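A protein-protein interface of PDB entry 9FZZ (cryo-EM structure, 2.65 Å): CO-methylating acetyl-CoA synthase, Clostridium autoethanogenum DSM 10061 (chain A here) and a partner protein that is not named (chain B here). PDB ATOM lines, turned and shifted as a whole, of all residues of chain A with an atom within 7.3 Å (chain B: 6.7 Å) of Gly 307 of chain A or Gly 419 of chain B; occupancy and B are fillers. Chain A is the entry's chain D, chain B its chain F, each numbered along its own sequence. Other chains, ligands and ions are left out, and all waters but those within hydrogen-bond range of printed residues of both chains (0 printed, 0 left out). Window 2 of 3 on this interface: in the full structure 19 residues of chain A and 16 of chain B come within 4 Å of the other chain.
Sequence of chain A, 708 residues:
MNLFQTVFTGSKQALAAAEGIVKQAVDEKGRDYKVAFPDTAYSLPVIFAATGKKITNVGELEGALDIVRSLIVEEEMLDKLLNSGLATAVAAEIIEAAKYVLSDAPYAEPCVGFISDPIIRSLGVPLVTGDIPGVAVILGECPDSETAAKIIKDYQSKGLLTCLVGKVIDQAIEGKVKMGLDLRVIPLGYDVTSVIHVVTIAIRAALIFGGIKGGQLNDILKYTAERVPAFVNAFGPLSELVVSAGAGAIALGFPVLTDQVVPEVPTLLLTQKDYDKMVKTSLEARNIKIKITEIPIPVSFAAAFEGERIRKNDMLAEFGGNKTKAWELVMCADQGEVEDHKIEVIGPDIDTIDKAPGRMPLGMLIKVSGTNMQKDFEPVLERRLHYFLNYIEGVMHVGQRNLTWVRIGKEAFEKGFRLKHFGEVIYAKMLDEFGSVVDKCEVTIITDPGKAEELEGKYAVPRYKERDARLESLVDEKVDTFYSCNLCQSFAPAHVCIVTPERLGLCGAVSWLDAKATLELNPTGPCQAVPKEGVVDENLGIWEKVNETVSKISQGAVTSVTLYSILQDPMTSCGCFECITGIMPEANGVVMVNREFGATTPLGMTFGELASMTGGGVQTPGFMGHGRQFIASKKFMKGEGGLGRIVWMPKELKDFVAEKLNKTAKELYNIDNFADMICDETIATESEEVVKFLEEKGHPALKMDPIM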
ATOM      1  N   ALA A 303      -6.662 -18.842 -17.503  1.00  0.00           N
ATOM      2  CA  ALA A 303      -6.514 -17.391 -17.484  1.00  0.00           C
ATOM      3  C   ALA A 303      -7.134 -16.721 -18.699  1.00  0.00           C
ATOM      4  O   ALA A 303      -7.457 -15.533 -18.637  1.00  0.00           O
ATOM      5  CB  ALA A 303      -5.031 -17.010 -17.378  1.00  0.00           C
ATOM      6  N   ALA A 304      -7.299 -17.447 -19.803  1.00  0.00           N
ATOM      7  CA  ALA A 304      -7.908 -16.880 -20.997  1.00  0.00           C
ATOM      8  C   ALA A 304      -9.403 -16.643 -20.842  1.00  0.00           C
ATOM      9  O   ALA A 304     -10.006 -16.008 -21.713  1.00  0.00           O
ATOM     10  CB  ALA A 304      -7.654 -17.792 -22.204  1.00  0.00           C
ATOM     11  N   PHE A 305     -10.016 -17.130 -19.762  1.00  0.00           N
ATOM     12  CA  PHE A 305     -11.454 -17.014 -19.560  1.00  0.00           C
ATOM     13  C   PHE A 305     -11.864 -15.667 -18.980  1.00  0.00           C
ATOM     14  O   PHE A 305     -13.061 -15.407 -18.837  1.00  0.00           O
ATOM     15  CB  PHE A 305     -11.951 -18.138 -18.644  1.00  0.00           C
ATOM     16  CG  PHE A 305     -11.667 -19.527 -19.164  1.00  0.00           C
ATOM     17  CD1 PHE A 305     -11.244 -19.724 -20.485  1.00  0.00           C
ATOM     18  CD2 PHE A 305     -11.823 -20.636 -18.339  1.00  0.00           C
ATOM     19  CE1 PHE A 305     -10.977 -21.011 -20.976  1.00  0.00           C
ATOM     20  CE2 PHE A 305     -11.566 -21.933 -18.809  1.00  0.00           C
ATOM     21  CZ  PHE A 305     -11.140 -22.121 -20.135  1.00  0.00           C
ATOM     22  N   GLU A 306     -10.900 -14.819 -18.648  1.00  0.00           N
ATOM     23  CA  GLU A 306     -11.207 -13.497 -18.132  1.00  0.00           C
ATOM     24  C   GLU A 306     -11.875 -12.644 -19.203  1.00  0.00           C
ATOM     25  O   GLU A 306     -11.601 -12.777 -20.399  1.00  0.00           O
ATOM     26  CB  GLU A 306      -9.931 -12.810 -17.645  1.00  0.00           C
ATOM     27  CG  GLU A 306     -10.177 -11.412 -17.068  1.00  0.00           C
ATOM     28  CD  GLU A 306      -8.891 -10.759 -16.600  1.00  0.00           C
ATOM     29  OE1 GLU A 306      -7.922 -11.497 -16.353  1.00  0.00           O
ATOM     30  OE2 GLU A 306      -8.846  -9.515 -16.494  1.00  0.00           O
ATOM     31  N   GLY A 307     -12.794 -11.787 -18.766  1.00  0.00           N
ATOM     32  CA  GLY A 307     -13.467 -10.880 -19.669  1.00  0.00           C
ATOM     33  C   GLY A 307     -14.593 -11.487 -20.471  1.00  0.00           C
ATOM     34  O   GLY A 307     -15.161 -10.798 -21.326  1.00  0.00           O
ATOM     35  N   GLU A 308     -14.926 -12.750 -20.234  1.00  0.00           N
ATOM     36  CA  GLU A 308     -16.028 -13.374 -20.947  1.00  0.00           C
ATOM     37  C   GLU A 308     -17.345 -12.734 -20.528  1.00  0.00           C
ATOM     38  O   GLU A 308     -17.599 -12.532 -19.336  1.00  0.00           O
ATOM     39  CB  GLU A 308     -16.057 -14.880 -20.684  1.00  0.00           C
ATOM     40  CG  GLU A 308     -17.271 -15.571 -21.319  1.00  0.00           C
ATOM     41  CD  GLU A 308     -17.339 -17.051 -20.983  1.00  0.00           C
ATOM     42  OE1 GLU A 308     -16.295 -17.615 -20.609  1.00  0.00           O
ATOM     43  OE2 GLU A 308     -18.436 -17.643 -21.081  1.00  0.00           O
ATOM     44  N   ARG A 309     -18.167 -12.385 -21.515  1.00  0.00           N
ATOM     45  CA  ARG A 309     -19.511 -11.868 -21.291  1.00  0.00           C
ATOM     46  C   ARG A 309     -20.504 -12.978 -21.614  1.00  0.00           C
ATOM     47  O   ARG A 309     -20.466 -13.551 -22.709  1.00  0.00           O
ATOM     48  CB  ARG A 309     -19.784 -10.634 -22.151  1.00  0.00           C
ATOM     49  CG  ARG A 309     -19.515  -9.320 -21.416  1.00  0.00           C
ATOM     50  CD  ARG A 309     -19.471  -8.155 -22.402  1.00  0.00           C
ATOM     51  NE  ARG A 309     -19.537  -6.860 -21.737  1.00  0.00           N
ATOM     52  CZ  ARG A 309     -18.522  -6.281 -21.108  1.00  0.00           C
ATOM     53  NH1 ARG A 309     -17.342  -6.869 -21.007  1.00  0.00           N
ATOM     54  NH2 ARG A 309     -18.696  -5.079 -20.558  1.00  0.00           N
ATOM     55  N   ILE A 310     -21.385 -13.280 -20.665  1.00  0.00           N
ATOM     56  CA  ILE A 310     -22.269 -14.434 -20.746  1.00  0.00           C
ATOM     57  C   ILE A 310     -23.708 -13.948 -20.660  1.00  0.00           C
ATOM     58  O   ILE A 310     -24.021 -13.019 -19.904  1.00  0.00           O
ATOM     59  CB  ILE A 310     -21.936 -15.461 -19.644  1.00  0.00           C
ATOM     60  CG1 ILE A 310     -22.992 -16.576 -19.606  1.00  0.00           C
ATOM     61  CG2 ILE A 310     -21.756 -14.763 -18.288  1.00  0.00           C
ATOM     62  CD1 ILE A 310     -22.646 -17.696 -18.628  1.00  0.00           C
ATOM     63  N   ASN A 390     -12.565 -14.592 -11.779  1.00  0.00           N
ATOM     64  CA  ASN A 390     -12.821 -14.380 -13.203  1.00  0.00           C
ATOM     65  C   ASN A 390     -12.153 -15.431 -14.079  1.00  0.00           C
ATOM     66  O   ASN A 390     -12.593 -15.647 -15.211  1.00  0.00           O
ATOM     67  CB  ASN A 390     -12.375 -12.982 -13.636  1.00  0.00           C
ATOM     68  CG  ASN A 390     -13.451 -11.929 -13.405  1.00  0.00           C
ATOM     69  OD1 ASN A 390     -13.203 -10.904 -12.781  1.00  0.00           O
ATOM     70  ND2 ASN A 390     -14.668 -12.191 -13.907  1.00  0.00           N
ATOM     71  N   TYR A 391     -11.110 -16.098 -13.585  1.00  0.00           N
ATOM     72  CA  TYR A 391     -10.482 -17.172 -14.348  1.00  0.00           C
ATOM     73  C   TYR A 391     -11.354 -18.411 -14.450  1.00  0.00           C
ATOM     74  O   TYR A 391     -11.040 -19.299 -15.249  1.00  0.00           O
ATOM     75  CB  TYR A 391      -9.134 -17.556 -13.728  1.00  0.00           C
ATOM     76  CG  TYR A 391      -8.051 -16.521 -13.917  1.00  0.00           C
ATOM     77  CD1 TYR A 391      -8.149 -15.545 -14.918  1.00  0.00           C
ATOM     78  CD2 TYR A 391      -6.924 -16.512 -13.100  1.00  0.00           C
ATOM     79  CE1 TYR A 391      -7.145 -14.587 -15.097  1.00  0.00           C
ATOM     80  CE2 TYR A 391      -5.910 -15.561 -13.265  1.00  0.00           C
ATOM     81  CZ  TYR A 391      -6.032 -14.606 -14.264  1.00  0.00           C
ATOM     82  OH  TYR A 391      -5.022 -13.672 -14.414  1.00  0.00           O
ATOM     83  N   MET A 396     -18.825 -14.593 -13.555  1.00  0.00           N
ATOM     84  CA  MET A 396     -18.246 -13.268 -13.744  1.00  0.00           C
ATOM     85  C   MET A 396     -18.467 -12.475 -12.471  1.00  0.00           C
ATOM     86  O   MET A 396     -19.615 -12.251 -12.081  1.00  0.00           O
ATOM     87  CB  MET A 396     -18.889 -12.558 -14.943  1.00  0.00           C
ATOM     88  CG  MET A 396     -18.648 -11.039 -14.968  1.00  0.00           C
ATOM     89  SD  MET A 396     -19.875 -10.176 -15.964  1.00  0.00           S
ATOM     90  CE  MET A 396     -19.572 -10.855 -17.583  1.00  0.00           C
ATOM     91  N   ALA B 415      -7.062 -11.541 -24.731  1.00  0.00           N
ATOM     92  CA  ALA B 415      -8.202 -12.448 -24.716  1.00  0.00           C
ATOM     93  C   ALA B 415      -9.364 -11.896 -23.908  1.00  0.00           C
ATOM     94  O   ALA B 415     -10.511 -12.289 -24.143  1.00  0.00           O
ATOM     95  CB  ALA B 415      -7.795 -13.817 -24.153  1.00  0.00           C
ATOM     96  N   VAL B 416      -9.087 -10.980 -22.980  1.00  0.00           N
ATOM     97  CA  VAL B 416     -10.147 -10.346 -22.207  1.00  0.00           C
ATOM     98  C   VAL B 416     -11.035  -9.508 -23.117  1.00  0.00           C
ATOM     99  O   VAL B 416     -12.237  -9.368 -22.863  1.00  0.00           O
ATOM    100  CB  VAL B 416      -9.534  -9.516 -21.060  1.00  0.00           C
ATOM    101  CG1 VAL B 416      -8.416  -8.604 -21.569  1.00  0.00           C
ATOM    102  CG2 VAL B 416     -10.600  -8.678 -20.351  1.00  0.00           C
ATOM    103  N   LEU B 417     -10.472  -8.942 -24.184  1.00  0.00           N
ATOM    104  CA  LEU B 417     -11.215  -8.041 -25.055  1.00  0.00           C
ATOM    105  C   LEU B 417     -12.321  -8.731 -25.844  1.00  0.00           C
ATOM    106  O   LEU B 417     -13.140  -8.039 -26.456  1.00  0.00           O
ATOM    107  CB  LEU B 417     -10.259  -7.351 -26.035  1.00  0.00           C
ATOM    108  CG  LEU B 417      -9.693  -5.999 -25.581  1.00  0.00           C
ATOM    109  CD1 LEU B 417      -8.900  -6.122 -24.286  1.00  0.00           C
ATOM    110  CD2 LEU B 417      -8.823  -5.416 -26.683  1.00  0.00           C
ATOM    111  N   LYS B 418     -12.366 -10.062 -25.857  1.00  0.00           N
ATOM    112  CA  LYS B 418     -13.356 -10.759 -26.673  1.00  0.00           C
ATOM    113  C   LYS B 418     -14.778 -10.411 -26.248  1.00  0.00           C
ATOM    114  O   LYS B 418     -15.633 -10.112 -27.090  1.00  0.00           O
ATOM    115  CB  LYS B 418     -13.127 -12.268 -26.591  1.00  0.00           C
ATOM    116  CG  LYS B 418     -13.982 -13.064 -27.575  1.00  0.00           C
ATOM    117  CD  LYS B 418     -13.673 -14.559 -27.468  1.00  0.00           C
ATOM    118  CE  LYS B 418     -14.313 -15.344 -28.619  1.00  0.00           C
ATOM    119  NZ  LYS B 418     -15.801 -15.140 -28.647  1.00  0.00           N
ATOM    120  N   GLY B 419     -15.044 -10.421 -24.943  1.00  0.00           N
ATOM    121  CA  GLY B 419     -16.382 -10.094 -24.474  1.00  0.00           C
ATOM    122  C   GLY B 419     -16.777  -8.663 -24.782  1.00  0.00           C
ATOM    123  O   GLY B 419     -17.882  -8.400 -25.256  1.00  0.00           O
ATOM    124  N   GLU B 420     -15.870  -7.720 -24.525  1.00  0.00           N
ATOM    125  CA  GLU B 420     -16.159  -6.313 -24.799  1.00  0.00           C
ATOM    126  C   GLU B 420     -16.354  -6.063 -26.289  1.00  0.00           C
ATOM    127  O   GLU B 420     -17.246  -5.310 -26.692  1.00  0.00           O
ATOM    128  CB  GLU B 420     -15.041  -5.427 -24.250  1.00  0.00           C
ATOM    129  CG  GLU B 420     -14.909  -5.492 -22.726  1.00  0.00           C
ATOM    130  CD  GLU B 420     -13.478  -5.260 -22.259  1.00  0.00           C
ATOM    131  OE1 GLU B 420     -12.550  -5.706 -22.960  1.00  0.00           O
ATOM    132  OE2 GLU B 420     -13.281  -4.629 -21.201  1.00  0.00           O
ATOM    133  N   LEU B 421     -15.516  -6.675 -27.125  1.00  0.00           N
ATOM    134  CA  LEU B 421     -15.655  -6.489 -28.568  1.00  0.00           C
ATOM    135  C   LEU B 421     -16.961  -7.078 -29.082  1.00  0.00           C
ATOM    136  O   LEU B 421     -17.626  -6.476 -29.930  1.00  0.00           O
ATOM    137  CB  LEU B 421     -14.462  -7.105 -29.298  1.00  0.00           C
ATOM    138  CG  LEU B 421     -13.146  -6.340 -29.111  1.00  0.00           C
ATOM    139  CD1 LEU B 421     -11.997  -7.111 -29.741  1.00  0.00           C
ATOM    140  CD2 LEU B 421     -13.240  -4.944 -29.710  1.00  0.00           C
ATOM    141  N   GLU B 422     -17.346  -8.254 -28.586  1.00  0.00           N
ATOM    142  CA  GLU B 422     -18.633  -8.820 -28.987  1.00  0.00           C
ATOM    143  C   GLU B 422     -19.790  -7.959 -28.490  1.00  0.00           C
ATOM    144  O   GLU B 422     -20.803  -7.805 -29.182  1.00  0.00           O
ATOM    145  CB  GLU B 422     -18.761 -10.256 -28.479  1.00  0.00           C
ATOM    146  CG  GLU B 422     -17.865 -11.234 -29.241  1.00  0.00           C
ATOM    147  CD  GLU B 422     -17.893 -12.636 -28.646  1.00  0.00           C
ATOM    148  OE1 GLU B 422     -18.305 -12.775 -27.480  1.00  0.00           O
ATOM    149  OE2 GLU B 422     -17.504 -13.596 -29.346  1.00  0.00           O
ATOM    150  N   GLU B 423     -19.653  -7.380 -27.295  1.00  0.00           N
ATOM    151  CA  GLU B 423     -20.690  -6.507 -26.759  1.00  0.00           C
ATOM    152  C   GLU B 423     -20.851  -5.252 -27.606  1.00  0.00           C
ATOM    153  O   GLU B 423     -21.971  -4.843 -27.925  1.00  0.00           O
ATOM    154  CB  GLU B 423     -20.346  -6.138 -25.313  1.00  0.00           C
ATOM    155  CG  GLU B 423     -21.312  -5.138 -24.652  1.00  0.00           C
ATOM    156  CD  GLU B 423     -22.333  -5.825 -23.753  1.00  0.00           C
ATOM    157  OE1 GLU B 423     -22.821  -6.907 -24.128  1.00  0.00           O
ATOM    158  OE2 GLU B 423     -22.633  -5.289 -22.666  1.00  0.00           O
ATOM    159  N   LEU B 424     -19.739  -4.624 -27.980  1.00  0.00           N
ATOM    160  CA  LEU B 424     -19.784  -3.386 -28.748  1.00  0.00           C
ATOM    161  C   LEU B 424     -19.946  -3.607 -30.245  1.00  0.00           C
ATOM    162  O   LEU B 424     -20.273  -2.654 -30.960  1.00  0.00           O
ATOM    163  CB  LEU B 424     -18.521  -2.554 -28.487  1.00  0.00           C
ATOM    164  CG  LEU B 424     -18.617  -1.567 -27.311  1.00  0.00           C
ATOM    165  CD1 LEU B 424     -18.714  -2.300 -25.976  1.00  0.00           C
ATOM    166  CD2 LEU B 424     -17.425  -0.616 -27.320  1.00  0.00           C
ATOM    167  N   ILE B 430     -16.086 -11.795 -33.633  1.00  0.00           N
ATOM    168  CA  ILE B 430     -14.772 -11.700 -33.011  1.00  0.00           C
ATOM    169  C   ILE B 430     -14.155 -13.088 -32.938  1.00  0.00           C
ATOM    170  O   ILE B 430     -14.775 -14.030 -32.430  1.00  0.00           O
ATOM    171  CB  ILE B 430     -14.873 -11.073 -31.613  1.00  0.00           C
ATOM    172  CG1 ILE B 430     -15.643  -9.740 -31.656  1.00  0.00           C
ATOM    173  CG2 ILE B 430     -13.476 -10.863 -31.023  1.00  0.00           C
ATOM    174  CD1 ILE B 430     -14.984  -8.677 -32.523  1.00  0.00           C
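Gly 307 of chain A touches two residues of chain B.
Of the printed residues of chain B, Glu 306 of chain A touches Ala 415 and Val 416.
Printed residues of chain A within 4 Å of Glu 420 of chain B: Arg 309 (3.3 Å).
Leu 424 of chain B touches none of the printed residues of chain A.
The nearest residue of chain B that does not touch Gly 307 of chain A is Glu 420 of chain B (4.5 Å).
The nearest residue of chain A that does not touch Gly 419 of chain B is Glu 308 of chain A (4.8 Å).
Among the printed residues, merely in contact across the chains: Arg 309 of chain A with Gly 419 of chain B, Arg 309 of chain A with Glu 420 of chain B, Glu 306 of chain A with Val 416 of chain B, Gly 307 of chain A with Gly 419 of chain B, Gly 307 of chain A with Val 416 of chain B, Glu 306 of chain A with Ala 415 of chain B and Ala 304 of chain A with Ala 415 of chain B.
The side-chain carboxylate (OE2) of Glu 423 of chain B lies within salt-bridge range of the guanidinium group (NE) of Arg 309 of chain A (3.6 Å).
Printed residues of chain B that touch a printed residue of chain A: Ala 415, Val 416, Gly 419, Glu 420 and Glu 423.
Among the printed residues, Asp or Glu carboxylates within 4 Å of a Lys or Arg side-chain nitrogen of the other chain: Arg 309 of chain A with Glu 423 of chain B (3.6 Å).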
